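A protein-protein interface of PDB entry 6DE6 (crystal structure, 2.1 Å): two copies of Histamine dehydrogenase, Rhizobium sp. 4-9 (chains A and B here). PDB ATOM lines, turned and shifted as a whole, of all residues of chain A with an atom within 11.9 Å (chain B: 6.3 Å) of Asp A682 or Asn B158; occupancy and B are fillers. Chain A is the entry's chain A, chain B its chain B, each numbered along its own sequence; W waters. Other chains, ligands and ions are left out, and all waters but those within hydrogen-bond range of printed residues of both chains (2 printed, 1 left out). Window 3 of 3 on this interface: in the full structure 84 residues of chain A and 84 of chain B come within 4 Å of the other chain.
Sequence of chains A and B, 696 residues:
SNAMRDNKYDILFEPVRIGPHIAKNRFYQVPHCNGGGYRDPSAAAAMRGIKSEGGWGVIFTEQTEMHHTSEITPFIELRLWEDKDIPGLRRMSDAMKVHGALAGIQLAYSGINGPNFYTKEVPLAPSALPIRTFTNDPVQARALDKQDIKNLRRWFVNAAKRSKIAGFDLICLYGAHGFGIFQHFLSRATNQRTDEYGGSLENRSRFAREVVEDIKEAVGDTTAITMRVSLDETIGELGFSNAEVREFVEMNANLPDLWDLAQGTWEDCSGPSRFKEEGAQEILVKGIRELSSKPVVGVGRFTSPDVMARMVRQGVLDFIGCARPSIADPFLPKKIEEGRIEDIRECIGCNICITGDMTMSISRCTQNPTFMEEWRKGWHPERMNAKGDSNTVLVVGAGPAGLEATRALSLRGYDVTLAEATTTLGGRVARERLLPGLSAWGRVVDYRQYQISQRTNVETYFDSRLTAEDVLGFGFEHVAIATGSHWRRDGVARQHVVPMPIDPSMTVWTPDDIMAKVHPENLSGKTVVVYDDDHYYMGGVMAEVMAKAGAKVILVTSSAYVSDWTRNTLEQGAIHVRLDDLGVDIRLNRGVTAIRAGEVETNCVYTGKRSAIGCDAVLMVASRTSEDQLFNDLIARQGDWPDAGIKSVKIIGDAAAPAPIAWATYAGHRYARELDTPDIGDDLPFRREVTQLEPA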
ATOM      1  N   ARG A 670       1.844 -12.248 -15.449  1.00  0.00           N
ATOM      2  CA  ARG A 670       1.276 -13.510 -15.024  1.00  0.00           C
ATOM      3  C   ARG A 670       1.678 -14.636 -15.974  1.00  0.00           C
ATOM      4  O   ARG A 670       2.066 -15.725 -15.527  1.00  0.00           O
ATOM      5  CB  ARG A 670      -0.248 -13.398 -14.923  1.00  0.00           C
ATOM      6  CG  ARG A 670      -0.903 -14.716 -14.565  1.00  0.00           C
ATOM      7  CD  ARG A 670      -2.414 -14.622 -14.290  1.00  0.00           C
ATOM      8  NE  ARG A 670      -2.911 -15.903 -13.816  1.00  0.00           N
ATOM      9  CZ  ARG A 670      -4.042 -16.070 -13.132  1.00  0.00           C
ATOM     10  NH1 ARG A 670      -4.820 -15.028 -12.852  1.00  0.00           N
ATOM     11  NH2 ARG A 670      -4.386 -17.291 -12.733  1.00  0.00           N
ATOM     12  N   GLU A 674       3.841 -17.996 -14.779  1.00  0.00           N
ATOM     13  CA  GLU A 674       3.178 -19.292 -14.717  1.00  0.00           C
ATOM     14  C   GLU A 674       3.738 -20.317 -15.701  1.00  0.00           C
ATOM     15  O   GLU A 674       3.503 -21.518 -15.526  1.00  0.00           O
ATOM     16  CB  GLU A 674       1.679 -19.112 -14.972  1.00  0.00           C
ATOM     17  CG  GLU A 674       0.949 -18.474 -13.815  1.00  0.00           C
ATOM     18  CD  GLU A 674      -0.560 -18.384 -14.050  1.00  0.00           C
ATOM     19  OE1 GLU A 674      -0.991 -18.306 -15.218  1.00  0.00           O
ATOM     20  OE2 GLU A 674      -1.306 -18.386 -13.062  1.00  0.00           O
ATOM     21  N   PRO A 678       3.802 -26.253 -12.228  1.00  0.00           N
ATOM     22  CA  PRO A 678       2.939 -27.434 -12.094  1.00  0.00           C
ATOM     23  C   PRO A 678       1.462 -27.078 -12.162  1.00  0.00           C
ATOM     24  O   PRO A 678       1.035 -26.015 -11.709  1.00  0.00           O
ATOM     25  CB  PRO A 678       3.287 -27.973 -10.700  1.00  0.00           C
ATOM     26  CG  PRO A 678       4.606 -27.337 -10.328  1.00  0.00           C
ATOM     27  CD  PRO A 678       4.636 -26.024 -11.033  1.00  0.00           C
ATOM     28  N   ASP A 679       0.677 -28.003 -12.708  1.00  0.00           N
ATOM     29  CA  ASP A 679      -0.778 -27.908 -12.640  1.00  0.00           C
ATOM     30  C   ASP A 679      -1.233 -27.809 -11.188  1.00  0.00           C
ATOM     31  O   ASP A 679      -0.806 -28.591 -10.334  1.00  0.00           O
ATOM     32  CB  ASP A 679      -1.398 -29.127 -13.324  1.00  0.00           C
ATOM     33  CG  ASP A 679      -2.928 -29.079 -13.393  1.00  0.00           C
ATOM     34  OD1 ASP A 679      -3.529 -27.984 -13.368  1.00  0.00           O
ATOM     35  OD2 ASP A 679      -3.526 -30.168 -13.534  1.00  0.00           O
ATOM     36  N   ILE A 680      -2.098 -26.833 -10.907  1.00  0.00           N
ATOM     37  CA  ILE A 680      -2.669 -26.675  -9.572  1.00  0.00           C
ATOM     38  C   ILE A 680      -4.091 -27.194  -9.500  1.00  0.00           C
ATOM     39  O   ILE A 680      -4.691 -27.204  -8.414  1.00  0.00           O
ATOM     40  CB  ILE A 680      -2.624 -25.201  -9.101  1.00  0.00           C
ATOM     41  CG1 ILE A 680      -3.516 -24.313  -9.972  1.00  0.00           C
ATOM     42  CG2 ILE A 680      -1.202 -24.674  -9.135  1.00  0.00           C
ATOM     43  CD1 ILE A 680      -3.634 -22.863  -9.477  1.00  0.00           C
ATOM     44  N   GLY A 681      -4.646 -27.638 -10.617  1.00  0.00           N
ATOM     45  CA  GLY A 681      -5.996 -28.181 -10.600  1.00  0.00           C
ATOM     46  C   GLY A 681      -6.986 -27.072 -10.315  1.00  0.00           C
ATOM     47  O   GLY A 681      -6.987 -26.026 -10.974  1.00  0.00           O
ATOM     48  N   ASP A 682      -7.854 -27.311  -9.338  1.00  0.00           N
ATOM     49  CA  ASP A 682      -8.821 -26.322  -8.893  1.00  0.00           C
ATOM     50  C   ASP A 682      -8.343 -25.545  -7.671  1.00  0.00           C
ATOM     51  O   ASP A 682      -9.147 -24.867  -7.020  1.00  0.00           O
ATOM     52  CB  ASP A 682     -10.151 -27.009  -8.613  1.00  0.00           C
ATOM     53  CG  ASP A 682     -10.826 -27.456  -9.890  1.00  0.00           C
ATOM     54  OD1 ASP A 682     -10.651 -26.768 -10.914  1.00  0.00           O
ATOM     55  OD2 ASP A 682     -11.504 -28.490  -9.877  1.00  0.00           O
ATOM     56  N   ASP A 683      -7.059 -25.636  -7.341  1.00  0.00           N
ATOM     57  CA  ASP A 683      -6.504 -24.832  -6.271  1.00  0.00           C
ATOM     58  C   ASP A 683      -6.411 -23.364  -6.696  1.00  0.00           C
ATOM     59  O   ASP A 683      -6.388 -23.020  -7.886  1.00  0.00           O
ATOM     60  CB  ASP A 683      -5.127 -25.357  -5.866  1.00  0.00           C
ATOM     61  CG  ASP A 683      -5.204 -26.725  -5.197  1.00  0.00           C
ATOM     62  OD1 ASP A 683      -6.291 -27.068  -4.668  1.00  0.00           O
ATOM     63  OD2 ASP A 683      -4.188 -27.458  -5.202  1.00  0.00           O
ATOM     64  N   LEU A 684      -6.374 -22.501  -5.701  1.00  0.00           N
ATOM     65  CA  LEU A 684      -6.253 -21.083  -5.970  1.00  0.00           C
ATOM     66  C   LEU A 684      -4.824 -20.744  -6.375  1.00  0.00           C
ATOM     67  O   LEU A 684      -3.879 -21.256  -5.781  1.00  0.00           O
ATOM     68  CB  LEU A 684      -6.630 -20.258  -4.745  1.00  0.00           C
ATOM     69  CG  LEU A 684      -8.111 -19.880  -4.698  1.00  0.00           C
ATOM     70  CD1 LEU A 684      -8.948 -21.119  -4.667  1.00  0.00           C
ATOM     71  CD2 LEU A 684      -8.387 -18.994  -3.492  1.00  0.00           C
ATOM     72  N   PRO A 685      -4.637 -19.867  -7.361  1.00  0.00           N
ATOM     73  CA  PRO A 685      -3.286 -19.408  -7.700  1.00  0.00           C
ATOM     74  C   PRO A 685      -2.771 -18.280  -6.819  1.00  0.00           C
ATOM     75  O   PRO A 685      -1.725 -17.704  -7.127  1.00  0.00           O
ATOM     76  CB  PRO A 685      -3.455 -18.957  -9.153  1.00  0.00           C
ATOM     77  CG  PRO A 685      -4.893 -18.473  -9.220  1.00  0.00           C
ATOM     78  CD  PRO A 685      -5.664 -19.276  -8.235  1.00  0.00           C
ATOM     79  N   PHE A 686      -3.473 -17.946  -5.740  1.00  0.00           N
ATOM     80  CA  PHE A 686      -2.996 -16.942  -4.807  1.00  0.00           C
ATOM     81  C   PHE A 686      -3.368 -17.379  -3.406  1.00  0.00           C
ATOM     82  O   PHE A 686      -4.366 -18.075  -3.205  1.00  0.00           O
ATOM     83  CB  PHE A 686      -3.574 -15.549  -5.096  1.00  0.00           C
ATOM     84  CG  PHE A 686      -5.094 -15.508  -5.165  1.00  0.00           C
ATOM     85  CD1 PHE A 686      -5.843 -15.308  -4.032  1.00  0.00           C
ATOM     86  CD2 PHE A 686      -5.755 -15.675  -6.366  1.00  0.00           C
ATOM     87  CE1 PHE A 686      -7.233 -15.261  -4.090  1.00  0.00           C
ATOM     88  CE2 PHE A 686      -7.145 -15.650  -6.428  1.00  0.00           C
ATOM     89  CZ  PHE A 686      -7.880 -15.435  -5.287  1.00  0.00           C
ATOM     90  N   ARG A 687      -2.559 -16.950  -2.444  1.00  0.00           N
ATOM     91  CA  ARG A 687      -2.869 -17.099  -1.036  1.00  0.00           C
ATOM     92  C   ARG A 687      -3.921 -16.080  -0.598  1.00  0.00           C
ATOM     93  O   ARG A 687      -4.050 -14.997  -1.169  1.00  0.00           O
ATOM     94  CB  ARG A 687      -1.623 -16.885  -0.191  1.00  0.00           C
ATOM     95  CG  ARG A 687      -0.508 -17.910  -0.405  1.00  0.00           C
ATOM     96  CD  ARG A 687       0.827 -17.301  -0.031  1.00  0.00           C
ATOM     97  NE  ARG A 687       1.404 -17.796   1.203  1.00  0.00           N
ATOM     98  CZ  ARG A 687       2.629 -17.466   1.618  1.00  0.00           C
ATOM     99  NH1 ARG A 687       3.391 -16.651   0.883  1.00  0.00           N
ATOM    100  NH2 ARG A 687       3.091 -17.937   2.767  1.00  0.00           N
ATOM    101  N   ARG A 688      -4.623 -16.412   0.481  1.00  0.00           N
ATOM    102  CA  ARG A 688      -5.646 -15.535   1.012  1.00  0.00           C
ATOM    103  C   ARG A 688      -5.913 -15.905   2.457  1.00  0.00           C
ATOM    104  O   ARG A 688      -5.792 -17.066   2.849  1.00  0.00           O
ATOM    105  CB  ARG A 688      -6.934 -15.617   0.193  1.00  0.00           C
ATOM    106  CG  ARG A 688      -7.520 -16.979   0.094  1.00  0.00           C
ATOM    107  CD  ARG A 688      -8.805 -16.946  -0.729  1.00  0.00           C
ATOM    108  NE  ARG A 688      -9.963 -16.476   0.030  1.00  0.00           N
ATOM    109  CZ  ARG A 688     -10.897 -17.265   0.566  1.00  0.00           C
ATOM    110  NH1 ARG A 688     -10.810 -18.586   0.483  1.00  0.00           N
ATOM    111  NH2 ARG A 688     -11.917 -16.725   1.217  1.00  0.00           N
ATOM    112  N   HIS B  67     -16.629 -19.464  -6.638  1.00  0.00           N
ATOM    113  CA  HIS B  67     -15.347 -19.617  -7.315  1.00  0.00           C
ATOM    114  C   HIS B  67     -14.599 -18.301  -7.428  1.00  0.00           C
ATOM    115  O   HIS B  67     -15.197 -17.243  -7.621  1.00  0.00           O
ATOM    116  CB  HIS B  67     -15.509 -20.212  -8.707  1.00  0.00           C
ATOM    117  CG  HIS B  67     -14.266 -20.866  -9.209  1.00  0.00           C
ATOM    118  ND1 HIS B  67     -13.452 -20.287 -10.155  1.00  0.00           N
ATOM    119  CD2 HIS B  67     -13.688 -22.042  -8.881  1.00  0.00           C
ATOM    120  CE1 HIS B  67     -12.426 -21.081 -10.391  1.00  0.00           C
ATOM    121  NE2 HIS B  67     -12.547 -22.153  -9.636  1.00  0.00           N
ATOM    122  N   HIS B  68     -13.280 -18.388  -7.325  1.00  0.00           N
ATOM    123  CA  HIS B  68     -12.443 -17.198  -7.350  1.00  0.00           C
ATOM    124  C   HIS B  68     -12.377 -16.531  -8.726  1.00  0.00           C
ATOM    125  O   HIS B  68     -11.845 -15.417  -8.825  1.00  0.00           O
ATOM    126  CB  HIS B  68     -11.048 -17.569  -6.847  1.00  0.00           C
ATOM    127  CG  HIS B  68     -10.400 -18.676  -7.623  1.00  0.00           C
ATOM    128  ND1 HIS B  68     -10.665 -20.010  -7.384  1.00  0.00           N
ATOM    129  CD2 HIS B  68      -9.517 -18.645  -8.652  1.00  0.00           C
ATOM    130  CE1 HIS B  68      -9.972 -20.753  -8.233  1.00  0.00           C
ATOM    131  NE2 HIS B  68      -9.260 -19.950  -9.008  1.00  0.00           N
ATOM    132  N   LEU B  80     -17.045 -19.487  -0.810  1.00  0.00           N
ATOM    133  CA  LEU B  80     -16.771 -20.907  -0.650  1.00  0.00           C
ATOM    134  C   LEU B  80     -15.809 -21.304  -1.771  1.00  0.00           C
ATOM    135  O   LEU B  80     -16.182 -21.955  -2.755  1.00  0.00           O
ATOM    136  CB  LEU B  80     -18.049 -21.743  -0.684  1.00  0.00           C
ATOM    137  CG  LEU B  80     -17.920 -23.243  -0.381  1.00  0.00           C
ATOM    138  CD1 LEU B  80     -17.093 -23.461   0.860  1.00  0.00           C
ATOM    139  CD2 LEU B  80     -19.320 -23.820  -0.177  1.00  0.00           C
ATOM    140  N   TRP B  81     -14.557 -20.883  -1.614  1.00  0.00           N
ATOM    141  CA  TRP B  81     -13.529 -21.081  -2.620  1.00  0.00           C
ATOM    142  C   TRP B  81     -12.566 -22.213  -2.286  1.00  0.00           C
ATOM    143  O   TRP B  81     -11.918 -22.739  -3.196  1.00  0.00           O
ATOM    144  CB  TRP B  81     -12.725 -19.795  -2.793  1.00  0.00           C
ATOM    145  CG  TRP B  81     -13.495 -18.625  -3.356  1.00  0.00           C
ATOM    146  CD1 TRP B  81     -14.740 -18.640  -3.908  1.00  0.00           C
ATOM    147  CD2 TRP B  81     -13.040 -17.276  -3.432  1.00  0.00           C
ATOM    148  NE1 TRP B  81     -15.083 -17.386  -4.344  1.00  0.00           N
ATOM    149  CE2 TRP B  81     -14.059 -16.525  -4.045  1.00  0.00           C
ATOM    150  CE3 TRP B  81     -11.861 -16.631  -3.050  1.00  0.00           C
ATOM    151  CZ2 TRP B  81     -13.942 -15.163  -4.268  1.00  0.00           C
ATOM    152  CZ3 TRP B  81     -11.742 -15.285  -3.276  1.00  0.00           C
ATOM    153  CH2 TRP B  81     -12.774 -14.560  -3.886  1.00  0.00           C
ATOM    154  N   ASN B 151     -15.376 -26.707 -16.789  1.00  0.00           N
ATOM    155  CA  ASN B 151     -14.768 -26.305 -15.526  1.00  0.00           C
ATOM    156  C   ASN B 151     -15.816 -25.715 -14.590  1.00  0.00           C
ATOM    157  O   ASN B 151     -15.898 -26.100 -13.425  1.00  0.00           O
ATOM    158  CB  ASN B 151     -13.639 -25.295 -15.765  1.00  0.00           C
ATOM    159  CG  ASN B 151     -12.440 -25.904 -16.523  1.00  0.00           C
ATOM    160  OD1 ASN B 151     -12.325 -27.121 -16.663  1.00  0.00           O
ATOM    161  ND2 ASN B 151     -11.534 -25.042 -16.980  1.00  0.00           N
ATOM    162  N   ARG B 153     -18.972 -26.161 -14.408  1.00  0.00           N
ATOM    163  CA  ARG B 153     -19.769 -27.250 -13.846  1.00  0.00           C
ATOM    164  C   ARG B 153     -19.018 -27.964 -12.733  1.00  0.00           C
ATOM    165  O   ARG B 153     -19.558 -28.190 -11.643  1.00  0.00           O
ATOM    166  CB  ARG B 153     -20.165 -28.241 -14.942  1.00  0.00           C
ATOM    167  CG  ARG B 153     -21.213 -27.681 -15.885  1.00  0.00           C
ATOM    168  CD  ARG B 153     -21.312 -28.495 -17.176  1.00  0.00           C
ATOM    169  NE  ARG B 153     -21.569 -29.902 -16.881  1.00  0.00           N
ATOM    170  CZ  ARG B 153     -21.655 -30.862 -17.792  1.00  0.00           C
ATOM    171  NH1 ARG B 153     -21.515 -30.577 -19.079  1.00  0.00           N
ATOM    172  NH2 ARG B 153     -21.888 -32.116 -17.412  1.00  0.00           N
ATOM    173  N   ARG B 154     -17.767 -28.336 -12.992  1.00  0.00           N
ATOM    174  CA  ARG B 154     -16.965 -28.962 -11.954  1.00  0.00           C
ATOM    175  C   ARG B 154     -16.871 -28.054 -10.736  1.00  0.00           C
ATOM    176  O   ARG B 154     -17.006 -28.521  -9.597  1.00  0.00           O
ATOM    177  CB  ARG B 154     -15.570 -29.304 -12.507  1.00  0.00           C
ATOM    178  CG  ARG B 154     -14.709 -30.101 -11.531  1.00  0.00           C
ATOM    179  CD  ARG B 154     -13.314 -30.513 -12.110  1.00  0.00           C
ATOM    180  NE  ARG B 154     -12.472 -29.340 -12.382  1.00  0.00           N
ATOM    181  CZ  ARG B 154     -12.315 -28.775 -13.571  1.00  0.00           C
ATOM    182  NH1 ARG B 154     -12.901 -29.271 -14.664  1.00  0.00           N
ATOM    183  NH2 ARG B 154     -11.539 -27.712 -13.672  1.00  0.00           N
ATOM    184  N   TRP B 155     -16.693 -26.742 -10.951  1.00  0.00           N
ATOM    185  CA  TRP B 155     -16.563 -25.815  -9.818  1.00  0.00           C
ATOM    186  C   TRP B 155     -17.833 -25.765  -8.978  1.00  0.00           C
ATOM    187  O   TRP B 155     -17.759 -25.658  -7.746  1.00  0.00           O
ATOM    188  CB  TRP B 155     -16.214 -24.408 -10.296  1.00  0.00           C
ATOM    189  CG  TRP B 155     -14.904 -24.312 -11.041  1.00  0.00           C
ATOM    190  CD1 TRP B 155     -13.845 -25.145 -10.926  1.00  0.00           C
ATOM    191  CD2 TRP B 155     -14.533 -23.319 -12.012  1.00  0.00           C
ATOM    192  NE1 TRP B 155     -12.821 -24.736 -11.751  1.00  0.00           N
ATOM    193  CE2 TRP B 155     -13.225 -23.621 -12.437  1.00  0.00           C
ATOM    194  CE3 TRP B 155     -15.173 -22.209 -12.553  1.00  0.00           C
ATOM    195  CZ2 TRP B 155     -12.547 -22.857 -13.391  1.00  0.00           C
ATOM    196  CZ3 TRP B 155     -14.493 -21.444 -13.510  1.00  0.00           C
ATOM    197  CH2 TRP B 155     -13.200 -21.784 -13.919  1.00  0.00           C
ATOM    198  N   PHE B 156     -19.008 -25.827  -9.623  1.00  0.00           N
ATOM    199  CA  PHE B 156     -20.258 -25.917  -8.873  1.00  0.00           C
ATOM    200  C   PHE B 156     -20.340 -27.223  -8.086  1.00  0.00           C
ATOM    201  O   PHE B 156     -20.778 -27.229  -6.925  1.00  0.00           O
ATOM    202  CB  PHE B 156     -21.467 -25.808  -9.810  1.00  0.00           C
ATOM    203  CG  PHE B 156     -21.950 -24.400 -10.013  1.00  0.00           C
ATOM    204  CD1 PHE B 156     -22.673 -23.763  -9.024  1.00  0.00           C
ATOM    205  CD2 PHE B 156     -21.658 -23.704 -11.187  1.00  0.00           C
ATOM    206  CE1 PHE B 156     -23.108 -22.470  -9.205  1.00  0.00           C
ATOM    207  CE2 PHE B 156     -22.080 -22.419 -11.370  1.00  0.00           C
ATOM    208  CZ  PHE B 156     -22.801 -21.792 -10.393  1.00  0.00           C
ATOM    209  N   VAL B 157     -19.930 -28.346  -8.698  1.00  0.00           N
ATOM    210  CA  VAL B 157     -19.932 -29.612  -7.968  1.00  0.00           C
ATOM    211  C   VAL B 157     -19.004 -29.522  -6.760  1.00  0.00           C
ATOM    212  O   VAL B 157     -19.353 -29.965  -5.656  1.00  0.00           O
ATOM    213  CB  VAL B 157     -19.547 -30.797  -8.881  1.00  0.00           C
ATOM    214  CG1 VAL B 157     -19.307 -32.053  -8.032  1.00  0.00           C
ATOM    215  CG2 VAL B 157     -20.631 -31.101  -9.871  1.00  0.00           C
ATOM    216  N   ASN B 158     -17.804 -28.957  -6.949  1.00  0.00           N
ATOM    217  CA  ASN B 158     -16.885 -28.786  -5.832  1.00  0.00           C
ATOM    218  C   ASN B 158     -17.537 -28.015  -4.696  1.00  0.00           C
ATOM    219  O   ASN B 158     -17.412 -28.394  -3.523  1.00  0.00           O
ATOM    220  CB  ASN B 158     -15.604 -28.077  -6.289  1.00  0.00           C
ATOM    221  CG  ASN B 158     -14.742 -28.957  -7.139  1.00  0.00           C
ATOM    222  OD1 ASN B 158     -14.992 -30.160  -7.236  1.00  0.00           O
ATOM    223  ND2 ASN B 158     -13.680 -28.389  -7.714  1.00  0.00           N
ATOM    224  N   ALA B 159     -18.230 -26.922  -5.028  1.00  0.00           N
ATOM    225  CA  ALA B 159     -18.870 -26.095  -4.004  1.00  0.00           C
ATOM    226  C   ALA B 159     -20.013 -26.842  -3.332  1.00  0.00           C
ATOM    227  O   ALA B 159     -20.244 -26.676  -2.132  1.00  0.00           O
ATOM    228  CB  ALA B 159     -19.391 -24.790  -4.619  1.00  0.00           C
ATOM    229  N   ALA B 160     -20.740 -27.661  -4.096  1.00  0.00           N
ATOM    230  CA  ALA B 160     -21.813 -28.473  -3.528  1.00  0.00           C
ATOM    231  C   ALA B 160     -21.269 -29.476  -2.530  1.00  0.00           C
ATOM    232  O   ALA B 160     -21.835 -29.659  -1.442  1.00  0.00           O
ATOM    233  CB  ALA B 160     -22.564 -29.211  -4.635  1.00  0.00           C
ATOM    234  N   LYS B 161     -20.149 -30.114  -2.865  1.00  0.00           N
ATOM    235  CA  LYS B 161     -19.541 -31.042  -1.928  1.00  0.00           C
ATOM    236  C   LYS B 161     -19.087 -30.322  -0.674  1.00  0.00           C
ATOM    237  O   LYS B 161     -19.275 -30.828   0.442  1.00  0.00           O
ATOM    238  CB  LYS B 161     -18.363 -31.762  -2.593  1.00  0.00           C
ATOM    239  CG  LYS B 161     -18.780 -32.714  -3.681  1.00  0.00           C
ATOM    240  CD  LYS B 161     -17.566 -33.418  -4.287  1.00  0.00           C
ATOM    241  CE  LYS B 161     -17.983 -34.403  -5.374  1.00  0.00           C
ATOM    242  NZ  LYS B 161     -16.801 -34.825  -6.204  1.00  0.00           N
ATOM    243  N   ARG B 162     -18.474 -29.141  -0.826  1.00  0.00           N
ATOM    244  CA  ARG B 162     -18.088 -28.372   0.360  1.00  0.00           C
ATOM    245  C   ARG B 162     -19.314 -27.954   1.160  1.00  0.00           C
ATOM    246  O   ARG B 162     -19.245 -27.818   2.388  1.00  0.00           O
ATOM    247  CB  ARG B 162     -17.266 -27.139  -0.031  1.00  0.00           C
ATOM    248  CG  ARG B 162     -15.861 -27.470  -0.553  1.00  0.00           C
ATOM    249  CD  ARG B 162     -14.951 -26.246  -0.589  1.00  0.00           C
ATOM    250  NE  ARG B 162     -13.571 -26.632  -0.868  1.00  0.00           N
ATOM    251  CZ  ARG B 162     -12.967 -26.553  -2.056  1.00  0.00           C
ATOM    252  NH1 ARG B 162     -13.597 -26.081  -3.128  1.00  0.00           N
ATOM    253  NH2 ARG B 162     -11.704 -26.950  -2.162  1.00  0.00           N
ATOM    254  N   SER B 163     -20.431 -27.695   0.475  1.00  0.00           N
ATOM    255  CA  SER B 163     -21.644 -27.277   1.177  1.00  0.00           C
ATOM    256  C   SER B 163     -22.180 -28.416   2.034  1.00  0.00           C
ATOM    257  O   SER B 163     -22.672 -28.193   3.142  1.00  0.00           O
ATOM    258  CB  SER B 163     -22.692 -26.809   0.169  1.00  0.00           C
ATOM    259  OG  SER B 163     -22.224 -25.664  -0.509  1.00  0.00           O
HETATM  260  O   HOH W   1     -10.240 -24.760  -4.166  1.00  0.00           O
HETATM  261  O   HOH W   2     -11.560 -23.911  -7.600  1.00  0.00           O
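The guanidinium group (NE) of Arg B154 lies within salt-bridge range of the side-chain carboxylate (OD2) of Asp A682, 2.8 Å away. The side-chain carboxylate of Asp A682 lies within hydrogen-bond range of the indole nitrogen of Trp B155, at 3.1 Å. The side-chain carboxylate (OD2) of Asp A682 is in hydrogen-bond range of the side-chain amide nitrogen (ND2) of Asn B158, 3.1 Å away.
The backbone carbonyl oxygen (O) of His B67 lies close to the indole nitrogen (NE1) of Trp B81 (3.3 Å). A ring nitrogen (NE2) of His B67 sits close to the indole nitrogen of Trp B155, 3.3 Å away. The guanidinium group (NH1) of Arg B154 sits at hydrogen-bond distance from the side-chain amide oxygen (OD1) of Asn B151 (3.0 Å).
His B68 touches Leu A684. Leu A684 touches Trp B81 (CD1 to O, 3.7 Å). NE2 of His B68 touches CD of Pro A685 (3.7 Å). Trp B81 touches Arg A688.
Of chain B, only Arg B154, Trp B155 and Asn B158 come within 4 Å of Asp A682. Of the printed residues of chain B, Leu A684 touches His B68 and Trp B81. Of the printed residues of chain B, Arg A688 touches Trp B81. Leu B80 touches none of the printed residues of chain A. No residue of chain A comes within 4 Å of Asn B151. Of the printed residues of chain A, Trp B155 touches Asp A682. No residue of chain A comes within 4 Å of Val B157. Of chain A, only Asp A682 comes within 4 Å of Asn B158. No residue of chain A comes within 4 Å of Ala B159. No residue of chain A comes within 4 Å of Ala B160. No residue of chain A comes within 4 Å of Lys B161. No residue of chain A comes within 4 Å of Arg B162. Ser B163 touches none of the printed residues of chain A. The nearest residue of chain B that does not touch Asp A682 is His B68 (4.4 Å). The nearest residue of chain A that does not touch Asn B158 is Asp A683 (7.2 Å). The nearest printed residue of chain B that does not touch Pro A685 is His B67 (7.3 Å).
Printed residues of chain B that touch a printed residue of chain A: His B68, Trp B81, Arg B154, Trp B155 and Asn B158. Hydrophobic or aromatic side chains of chain B that line the printed part of chain A: His B68, Trp B81 and Trp B155. Among the printed residues, 7 pairs touch across the chains. Among the printed residues, Asp or Glu carboxylates within 4 Å of a Lys or Arg side-chain nitrogen of the other chain: Asp A682 with Arg B154 (2.8 Å).
No position is printed for both chains. Of the 7 pairs that touch across the chains among the printed residues, none has its exchanged pair printed and touching as well.
Water W2 lies within hydrogen-bond range of the backbone carbonyl oxygen of Asp A682 (2.7 Å) and a ring nitrogen (NE2) of His B67 (2.9 Å). Water W1 lies within hydrogen-bond range of O of Trp B81, O of Asp A682 and NH2 of Arg B162.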
